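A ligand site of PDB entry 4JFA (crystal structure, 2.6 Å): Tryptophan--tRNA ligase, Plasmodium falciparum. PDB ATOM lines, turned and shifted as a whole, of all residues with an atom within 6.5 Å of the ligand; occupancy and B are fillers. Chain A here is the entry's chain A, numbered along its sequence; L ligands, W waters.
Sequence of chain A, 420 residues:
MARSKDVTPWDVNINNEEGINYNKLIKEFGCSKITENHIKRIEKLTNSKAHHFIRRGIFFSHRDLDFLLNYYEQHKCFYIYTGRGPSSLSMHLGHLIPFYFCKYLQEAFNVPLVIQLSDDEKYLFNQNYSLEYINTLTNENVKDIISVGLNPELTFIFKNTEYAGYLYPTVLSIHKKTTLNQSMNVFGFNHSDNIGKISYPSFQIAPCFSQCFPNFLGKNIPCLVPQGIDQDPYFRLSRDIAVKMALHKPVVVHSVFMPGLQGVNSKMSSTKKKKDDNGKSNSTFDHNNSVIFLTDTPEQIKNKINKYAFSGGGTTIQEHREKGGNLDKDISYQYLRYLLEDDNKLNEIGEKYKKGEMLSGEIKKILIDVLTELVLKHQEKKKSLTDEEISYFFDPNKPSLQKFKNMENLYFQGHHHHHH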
ATOM      1  N   TYR A  81       3.351 -11.627 -17.352  1.00  0.00           N
ATOM      2  CA  TYR A  81       3.844 -10.911 -16.178  1.00  0.00           C
ATOM      3  C   TYR A  81       5.229 -11.393 -15.816  1.00  0.00           C
ATOM      4  O   TYR A  81       5.449 -12.591 -15.601  1.00  0.00           O
ATOM      5  CB  TYR A  81       2.886 -11.048 -14.992  1.00  0.00           C
ATOM      6  CG  TYR A  81       3.512 -10.777 -13.630  1.00  0.00           C
ATOM      7  CD1 TYR A  81       4.213  -9.606 -13.375  1.00  0.00           C
ATOM      8  CD2 TYR A  81       3.374 -11.696 -12.590  1.00  0.00           C
ATOM      9  CE1 TYR A  81       4.771  -9.359 -12.137  1.00  0.00           C
ATOM     10  CE2 TYR A  81       3.931 -11.449 -11.352  1.00  0.00           C
ATOM     11  CZ  TYR A  81       4.628 -10.279 -11.130  1.00  0.00           C
ATOM     12  OH  TYR A  81       5.177 -10.030  -9.889  1.00  0.00           O
ATOM     13  N   THR A  82       6.176 -10.458 -15.753  1.00  0.00           N
ATOM     14  CA  THR A  82       7.489 -10.780 -15.219  1.00  0.00           C
ATOM     15  C   THR A  82       8.011  -9.587 -14.431  1.00  0.00           C
ATOM     16  O   THR A  82       7.388  -8.520 -14.422  1.00  0.00           O
ATOM     17  CB  THR A  82       8.486 -11.173 -16.326  1.00  0.00           C
ATOM     18  OG1 THR A  82       9.603 -11.858 -15.746  1.00  0.00           O
ATOM     19  CG2 THR A  82       8.977  -9.948 -17.091  1.00  0.00           C
ATOM     20  N   GLY A  83       9.126  -9.774 -13.754  1.00  0.00           N
ATOM     21  CA  GLY A  83       9.645  -8.726 -12.890  1.00  0.00           C
ATOM     22  C   GLY A  83      11.152  -8.648 -12.829  1.00  0.00           C
ATOM     23  O   GLY A  83      11.867  -9.551 -13.276  1.00  0.00           O
ATOM     24  N   ARG A  84      11.636  -7.555 -12.241  1.00  0.00           N
ATOM     25  CA  ARG A  84      13.061  -7.311 -12.106  1.00  0.00           C
ATOM     26  C   ARG A  84      13.322  -6.683 -10.746  1.00  0.00           C
ATOM     27  O   ARG A  84      12.635  -5.735 -10.346  1.00  0.00           O
ATOM     28  CB  ARG A  84      13.542  -6.376 -13.218  1.00  0.00           C
ATOM     29  CG  ARG A  84      14.813  -5.596 -12.896  1.00  0.00           C
ATOM     30  CD  ARG A  84      16.036  -6.486 -12.846  1.00  0.00           C
ATOM     31  NE  ARG A  84      17.227  -5.741 -12.422  1.00  0.00           N
ATOM     32  CZ  ARG A  84      18.384  -6.297 -12.096  1.00  0.00           C
ATOM     33  NH1 ARG A  84      18.526  -7.613 -12.155  1.00  0.00           N
ATOM     34  NH2 ARG A  84      19.405  -5.538 -11.723  1.00  0.00           N
ATOM     35  N   GLY A  85      14.304  -7.217 -10.024  1.00  0.00           N
ATOM     36  CA  GLY A  85      14.710  -6.645  -8.757  1.00  0.00           C
ATOM     37  C   GLY A  85      15.933  -5.760  -8.954  1.00  0.00           C
ATOM     38  O   GLY A  85      17.032  -6.267  -9.177  1.00  0.00           O
ATOM     39  N   PRO A  86      15.745  -4.434  -8.852  1.00  0.00           N
ATOM     40  CA  PRO A  86      16.816  -3.467  -9.089  1.00  0.00           C
ATOM     41  C   PRO A  86      17.848  -3.459  -7.972  1.00  0.00           C
ATOM     42  O   PRO A  86      17.863  -2.550  -7.138  1.00  0.00           O
ATOM     43  CB  PRO A  86      16.078  -2.126  -9.130  1.00  0.00           C
ATOM     44  CG  PRO A  86      14.891  -2.347  -8.244  1.00  0.00           C
ATOM     45  CD  PRO A  86      14.486  -3.775  -8.444  1.00  0.00           C
ATOM     46  N   SER A  87      18.709  -4.474  -7.958  1.00  0.00           N
ATOM     47  CA  SER A  87      19.701  -4.636  -6.900  1.00  0.00           C
ATOM     48  C   SER A  87      21.064  -4.083  -7.340  1.00  0.00           C
ATOM     49  O   SER A  87      21.985  -3.987  -6.524  1.00  0.00           O
ATOM     50  CB  SER A  87      19.832  -6.109  -6.524  1.00  0.00           C
ATOM     51  OG  SER A  87      20.172  -6.889  -7.657  1.00  0.00           O
ATOM     52  N   GLN A 116       6.867  -5.874 -13.300  1.00  0.00           N
ATOM     53  CA  GLN A 116       7.007  -5.332 -11.959  1.00  0.00           C
ATOM     54  C   GLN A 116       8.464  -5.001 -11.650  1.00  0.00           C
ATOM     55  O   GLN A 116       9.350  -5.824 -11.847  1.00  0.00           O
ATOM     56  CB  GLN A 116       6.499  -6.329 -10.910  1.00  0.00           C
ATOM     57  CG  GLN A 116       6.807  -5.938  -9.473  1.00  0.00           C
ATOM     58  CD  GLN A 116       6.234  -6.906  -8.458  1.00  0.00           C
ATOM     59  OE1 GLN A 116       6.797  -7.976  -8.223  1.00  0.00           O
ATOM     60  NE2 GLN A 116       5.100  -6.539  -7.863  1.00  0.00           N
ATOM     61  N   LEU A 117       8.707  -3.788 -11.171  1.00  0.00           N
ATOM     62  CA  LEU A 117      10.011  -3.489 -10.598  1.00  0.00           C
ATOM     63  C   LEU A 117       9.905  -3.436  -9.077  1.00  0.00           C
ATOM     64  O   LEU A 117       9.313  -2.525  -8.497  1.00  0.00           O
ATOM     65  CB  LEU A 117      10.609  -2.205 -11.181  1.00  0.00           C
ATOM     66  CG  LEU A 117      11.421  -2.478 -12.448  1.00  0.00           C
ATOM     67  CD1 LEU A 117      10.584  -2.214 -13.695  1.00  0.00           C
ATOM     68  CD2 LEU A 117      12.711  -1.692 -12.481  1.00  0.00           C
ATOM     69  N   SER A 118      10.483  -4.452  -8.438  1.00  0.00           N
ATOM     70  CA  SER A 118      10.374  -4.626  -7.001  1.00  0.00           C
ATOM     71  C   SER A 118      11.434  -3.824  -6.260  1.00  0.00           C
ATOM     72  O   SER A 118      12.359  -4.390  -5.658  1.00  0.00           O
ATOM     73  CB  SER A 118      10.483  -6.106  -6.643  1.00  0.00           C
ATOM     74  OG  SER A 118      11.602  -6.709  -7.266  1.00  0.00           O
ATOM     75  N   GLU A 121      11.232  -4.589  -2.536  1.00  0.00           N
ATOM     76  CA  GLU A 121      11.982  -5.792  -2.180  1.00  0.00           C
ATOM     77  C   GLU A 121      13.437  -5.457  -1.926  1.00  0.00           C
ATOM     78  O   GLU A 121      13.968  -5.717  -0.837  1.00  0.00           O
ATOM     79  CB  GLU A 121      11.870  -6.845  -3.281  1.00  0.00           C
ATOM     80  CG  GLU A 121      12.654  -8.126  -2.992  1.00  0.00           C
ATOM     81  CD  GLU A 121      12.806  -9.020  -4.215  1.00  0.00           C
ATOM     82  OE1 GLU A 121      12.492  -8.560  -5.335  1.00  0.00           O
ATOM     83  OE2 GLU A 121      13.239 -10.182  -4.044  1.00  0.00           O
ATOM     84  N   LYS A 122      14.088  -4.883  -2.928  1.00  0.00           N
ATOM     85  CA  LYS A 122      15.515  -4.564  -2.819  1.00  0.00           C
ATOM     86  C   LYS A 122      15.823  -3.548  -1.718  1.00  0.00           C
ATOM     87  O   LYS A 122      16.901  -3.563  -1.148  1.00  0.00           O
ATOM     88  CB  LYS A 122      16.066  -4.098  -4.175  1.00  0.00           C
ATOM     89  CG  LYS A 122      15.996  -5.165  -5.251  1.00  0.00           C
ATOM     90  CD  LYS A 122      16.437  -6.511  -4.707  1.00  0.00           C
ATOM     91  CE  LYS A 122      16.229  -7.634  -5.715  1.00  0.00           C
ATOM     92  NZ  LYS A 122      16.488  -8.975  -5.120  1.00  0.00           N
ATOM     93  N   ASN A 160       6.618  -0.893  -7.523  1.00  0.00           N
ATOM     94  CA  ASN A 160       5.782  -1.204  -6.370  1.00  0.00           C
ATOM     95  C   ASN A 160       5.587   0.015  -5.473  1.00  0.00           C
ATOM     96  O   ASN A 160       4.497   0.231  -4.944  1.00  0.00           O
ATOM     97  CB  ASN A 160       6.374  -2.373  -5.563  1.00  0.00           C
ATOM     98  CG  ASN A 160       6.185  -3.716  -6.251  1.00  0.00           C
ATOM     99  OD1 ASN A 160       5.384  -3.850  -7.179  1.00  0.00           O
ATOM    100  ND2 ASN A 160       6.922  -4.723  -5.796  1.00  0.00           N
ATOM    101  N   TYR A 200       6.726  -8.920   1.668  1.00  0.00           N
ATOM    102  CA  TYR A 200       6.963  -8.757   0.218  1.00  0.00           C
ATOM    103  C   TYR A 200       6.367  -9.787  -0.748  1.00  0.00           C
ATOM    104  O   TYR A 200       5.769  -9.392  -1.758  1.00  0.00           O
ATOM    105  CB  TYR A 200       8.451  -8.546  -0.101  1.00  0.00           C
ATOM    106  CG  TYR A 200       8.693  -8.614  -1.593  1.00  0.00           C
ATOM    107  CD1 TYR A 200       9.305  -9.720  -2.160  1.00  0.00           C
ATOM    108  CD2 TYR A 200       8.263  -7.605  -2.431  1.00  0.00           C
ATOM    109  CE1 TYR A 200       9.507  -9.802  -3.532  1.00  0.00           C
ATOM    110  CE2 TYR A 200       8.460  -7.674  -3.796  1.00  0.00           C
ATOM    111  CZ  TYR A 200       9.077  -8.767  -4.337  1.00  0.00           C
ATOM    112  OH  TYR A 200       9.278  -8.840  -5.693  1.00  0.00           O
ATOM    113  N   PHE A 203       3.354  -9.219  -2.719  1.00  0.00           N
ATOM    114  CA  PHE A 203       3.415  -8.149  -3.715  1.00  0.00           C
ATOM    115  C   PHE A 203       3.926  -8.647  -5.058  1.00  0.00           C
ATOM    116  O   PHE A 203       3.572  -8.109  -6.098  1.00  0.00           O
ATOM    117  CB  PHE A 203       4.278  -6.986  -3.210  1.00  0.00           C
ATOM    118  CG  PHE A 203       3.624  -6.182  -2.122  1.00  0.00           C
ATOM    119  CD1 PHE A 203       2.999  -4.975  -2.415  1.00  0.00           C
ATOM    120  CD2 PHE A 203       3.657  -6.617  -0.808  1.00  0.00           C
ATOM    121  CE1 PHE A 203       2.399  -4.230  -1.414  1.00  0.00           C
ATOM    122  CE2 PHE A 203       3.063  -5.867   0.204  1.00  0.00           C
ATOM    123  CZ  PHE A 203       2.427  -4.674  -0.103  1.00  0.00           C
ATOM    124  N   GLN A 204       4.773  -9.681  -5.036  1.00  0.00           N
ATOM    125  CA  GLN A 204       5.257 -10.289  -6.258  1.00  0.00           C
ATOM    126  C   GLN A 204       4.204 -11.243  -6.827  1.00  0.00           C
ATOM    127  O   GLN A 204       4.121 -11.460  -8.038  1.00  0.00           O
ATOM    128  CB  GLN A 204       6.578 -11.026  -6.017  1.00  0.00           C
ATOM    129  CG  GLN A 204       7.130 -11.733  -7.246  1.00  0.00           C
ATOM    130  CD  GLN A 204       8.599 -12.088  -7.118  1.00  0.00           C
ATOM    131  OE1 GLN A 204       9.371 -11.373  -6.479  1.00  0.00           O
ATOM    132  NE2 GLN A 204       8.992 -13.206  -7.721  1.00  0.00           N
ATOM    133  N   VAL A 225       3.625 -16.280 -16.623  1.00  0.00           N
ATOM    134  CA  VAL A 225       4.766 -15.793 -15.872  1.00  0.00           C
ATOM    135  C   VAL A 225       6.046 -16.544 -16.269  1.00  0.00           C
ATOM    136  O   VAL A 225       6.302 -17.659 -15.793  1.00  0.00           O
ATOM    137  CB  VAL A 225       4.538 -15.921 -14.353  1.00  0.00           C
ATOM    138  CG1 VAL A 225       5.604 -15.176 -13.582  1.00  0.00           C
ATOM    139  CG2 VAL A 225       3.159 -15.389 -13.982  1.00  0.00           C
ATOM    140  N   PRO A 226       6.824 -15.949 -17.191  1.00  0.00           N
ATOM    141  CA  PRO A 226       8.168 -16.427 -17.529  1.00  0.00           C
ATOM    142  C   PRO A 226       9.129 -15.992 -16.434  1.00  0.00           C
ATOM    143  O   PRO A 226       9.078 -14.825 -16.025  1.00  0.00           O
ATOM    144  CB  PRO A 226       8.489 -15.682 -18.838  1.00  0.00           C
ATOM    145  CG  PRO A 226       7.182 -15.116 -19.316  1.00  0.00           C
ATOM    146  CD  PRO A 226       6.389 -14.857 -18.072  1.00  0.00           C
ATOM    147  N   GLN A 227       9.986 -16.885 -15.982  1.00  0.00           N
ATOM    148  CA  GLN A 227      10.831 -16.592 -14.831  1.00  0.00           C
ATOM    149  C   GLN A 227      12.074 -17.471 -14.771  1.00  0.00           C
ATOM    150  O   GLN A 227      12.142 -18.533 -15.391  1.00  0.00           O
ATOM    151  CB  GLN A 227      10.025 -16.792 -13.550  1.00  0.00           C
ATOM    152  CG  GLN A 227       9.650 -18.249 -13.273  1.00  0.00           C
ATOM    153  CD  GLN A 227       8.436 -18.391 -12.379  1.00  0.00           C
ATOM    154  OE1 GLN A 227       7.366 -17.860 -12.676  1.00  0.00           O
ATOM    155  NE2 GLN A 227       8.607 -19.109 -11.276  1.00  0.00           N
ATOM    156  N   GLY A 228      13.070 -17.007 -14.016  1.00  0.00           N
ATOM    157  CA  GLY A 228      14.191 -17.852 -13.653  1.00  0.00           C
ATOM    158  C   GLY A 228      13.677 -18.928 -12.726  1.00  0.00           C
ATOM    159  O   GLY A 228      12.667 -18.735 -12.040  1.00  0.00           O
ATOM    160  N   ASP A 230      14.587 -19.903  -9.977  1.00  0.00           N
ATOM    161  CA  ASP A 230      14.721 -19.596  -8.553  1.00  0.00           C
ATOM    162  C   ASP A 230      13.580 -18.716  -8.032  1.00  0.00           C
ATOM    163  O   ASP A 230      13.556 -18.360  -6.853  1.00  0.00           O
ATOM    164  CB  ASP A 230      16.066 -18.914  -8.296  1.00  0.00           C
ATOM    165  CG  ASP A 230      16.229 -17.629  -9.087  1.00  0.00           C
ATOM    166  OD1 ASP A 230      16.857 -16.686  -8.576  1.00  0.00           O
ATOM    167  OD2 ASP A 230      15.721 -17.560 -10.230  1.00  0.00           O
ATOM    168  N   GLN A 231      12.648 -18.357  -8.913  1.00  0.00           N
ATOM    169  CA  GLN A 231      11.499 -17.552  -8.524  1.00  0.00           C
ATOM    170  C   GLN A 231      10.302 -18.429  -8.231  1.00  0.00           C
ATOM    171  O   GLN A 231       9.260 -17.943  -7.774  1.00  0.00           O
ATOM    172  CB  GLN A 231      11.156 -16.543  -9.641  1.00  0.00           C
ATOM    173  CG  GLN A 231      12.229 -15.501  -9.903  1.00  0.00           C
ATOM    174  CD  GLN A 231      12.494 -14.618  -8.696  1.00  0.00           C
ATOM    175  OE1 GLN A 231      11.573 -14.079  -8.098  1.00  0.00           O
ATOM    176  NE2 GLN A 231      13.767 -14.488  -8.333  1.00  0.00           N
ATOM    177  N   TYR A 234       7.725 -18.348  -5.116  1.00  0.00           N
ATOM    178  CA  TYR A 234       6.722 -17.290  -5.167  1.00  0.00           C
ATOM    179  C   TYR A 234       5.454 -17.769  -5.850  1.00  0.00           C
ATOM    180  O   TYR A 234       4.336 -17.524  -5.379  1.00  0.00           O
ATOM    181  CB  TYR A 234       7.251 -16.081  -5.940  1.00  0.00           C
ATOM    182  CG  TYR A 234       8.318 -15.286  -5.227  1.00  0.00           C
ATOM    183  CD1 TYR A 234       9.659 -15.440  -5.539  1.00  0.00           C
ATOM    184  CD2 TYR A 234       7.982 -14.353  -4.245  1.00  0.00           C
ATOM    185  CE1 TYR A 234      10.638 -14.698  -4.900  1.00  0.00           C
ATOM    186  CE2 TYR A 234       8.949 -13.617  -3.604  1.00  0.00           C
ATOM    187  CZ  TYR A 234      10.279 -13.785  -3.930  1.00  0.00           C
ATOM    188  OH  TYR A 234      11.236 -13.046  -3.284  1.00  0.00           O
ATOM    189  N   PHE A 235       5.634 -18.467  -6.965  1.00  0.00           N
ATOM    190  CA  PHE A 235       4.528 -18.797  -7.854  1.00  0.00           C
ATOM    191  C   PHE A 235       3.996 -20.205  -7.652  1.00  0.00           C
ATOM    192  O   PHE A 235       2.920 -20.552  -8.149  1.00  0.00           O
ATOM    193  CB  PHE A 235       4.943 -18.525  -9.304  1.00  0.00           C
ATOM    194  CG  PHE A 235       5.407 -17.114  -9.528  1.00  0.00           C
ATOM    195  CD1 PHE A 235       4.495 -16.068  -9.478  1.00  0.00           C
ATOM    196  CD2 PHE A 235       6.740 -16.829  -9.765  1.00  0.00           C
ATOM    197  CE1 PHE A 235       4.915 -14.758  -9.673  1.00  0.00           C
ATOM    198  CE2 PHE A 235       7.160 -15.518  -9.960  1.00  0.00           C
ATOM    199  CZ  PHE A 235       6.239 -14.490  -9.914  1.00  0.00           C
HETATM  200  N1  LIG L   1      12.143 -10.739  -7.165  1.00  0.00           N
HETATM  201  C1  LIG L   1      12.747 -10.879  -8.477  1.00  0.00           C
HETATM  202  C2  LIG L   1      14.259 -10.726  -8.410  1.00  0.00           C
HETATM  203  O1  LIG L   1      14.994 -11.421  -9.115  1.00  0.00           O
HETATM  204  C3  LIG L   1      12.156  -9.849  -9.447  1.00  0.00           C
HETATM  205  C4  LIG L   1      10.697 -10.081  -9.736  1.00  0.00           C
HETATM  206  C5  LIG L   1       9.635  -9.360  -9.275  1.00  0.00           C
HETATM  207  C6  LIG L   1      10.143 -11.126 -10.553  1.00  0.00           C
HETATM  208  N2  LIG L   1       8.460  -9.880  -9.756  1.00  0.00           N
HETATM  209  C7  LIG L   1       8.744 -10.967 -10.537  1.00  0.00           C
HETATM  210  C8  LIG L   1      10.704 -12.173 -11.294  1.00  0.00           C
HETATM  211  C9  LIG L   1       7.892 -11.820 -11.243  1.00  0.00           C
HETATM  212  C10 LIG L   1       9.859 -13.021 -11.989  1.00  0.00           C
HETATM  213  C11 LIG L   1       8.462 -12.845 -11.955  1.00  0.00           C
HETATM  214  O2  LIG L   1      14.783  -9.912  -7.658  1.00  0.00           O
HETATM  215  O   HOH W   1      15.908  -9.338 -10.813  1.00  0.00           O
HETATM  216  O   HOH W   2      17.353 -12.775  -8.410  1.00  0.00           O
HETATM  217  O   HOH W   3      14.447 -12.716 -11.346  1.00  0.00           O
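Water W1 lies within hydrogen-bond range of the backbone NH of Gly 85, an oxygen (O1) of the ligand and the guanidinium group of Arg 84.
A nitrogen (N2) of the ligand sits at hydrogen-bond distance from the side-chain hydroxyl (OH) of Tyr 81, at 3.3 Å. The side-chain amide nitrogen of Gln 231 lies within hydrogen-bond range of an oxygen (O1) of the ligand (3.4 Å). An oxygen (O2) of the ligand is in salt-bridge range of the side-chain amino group (NZ) of Lys 122, at 3.2 Å. OE1 of Gln 204 is in hydrogen-bond range of N1 of the ligand. A nitrogen (N2) of the ligand is in hydrogen-bond range of the side-chain amide oxygen (OE1) of Gln 116. The side-chain carboxylate (OE1) of Glu 121 is in salt-bridge range of a nitrogen (N1) of the ligand (2.9 Å).
Merely in contact with the ligand: Gly 83, Phe 235, Gly 85, Arg 84, Tyr 200, Ser 118 and Thr 82. Hydrophobic or aromatic side chains that line the ligand: Tyr 81 and Phe 235. 13 residues have an atom within 4 Å of the ligand: Tyr 81, Thr 82, Gly 83, Arg 84, Gly 85, Gln 116, Ser 118, Glu 121, Lys 122, Tyr 200, Gln 204, Gln 231 and Phe 235. The nearest printed residue that does not touch the ligand is Val 225 (4.03 Å).
The backbone carbonyl oxygen (O) of Gln 116 is in hydrogen-bond range of the backbone NH (N) of Arg 84 (2.9 Å). OE1 of Gln 231 is in hydrogen-bond range of NE2 of Gln 204 (2.8 Å). The backbone NH (N) of Gln 116 lies within hydrogen-bond range of the backbone carbonyl oxygen (O) of Thr 82 (2.9 Å). OE2 of Glu 121 lies within salt-bridge range of NZ of Lys 122 (3.6 Å). The side-chain amide nitrogen (NE2) of Gln 116 lies within hydrogen-bond range of the backbone carbonyl oxygen (O) of Phe 203 (2.8 Å). The side-chain hydroxyl (OH) of Tyr 81 is in hydrogen-bond range of the side-chain amide oxygen (OE1) of Gln 116. The backbone carbonyl oxygen of Arg 84 lies within hydrogen-bond range of the backbone NH of Ser 118 (3.1 Å). The side-chain amide oxygen of Gln 204 lies within hydrogen-bond range of the side-chain hydroxyl of Tyr 200 (2.7 Å).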
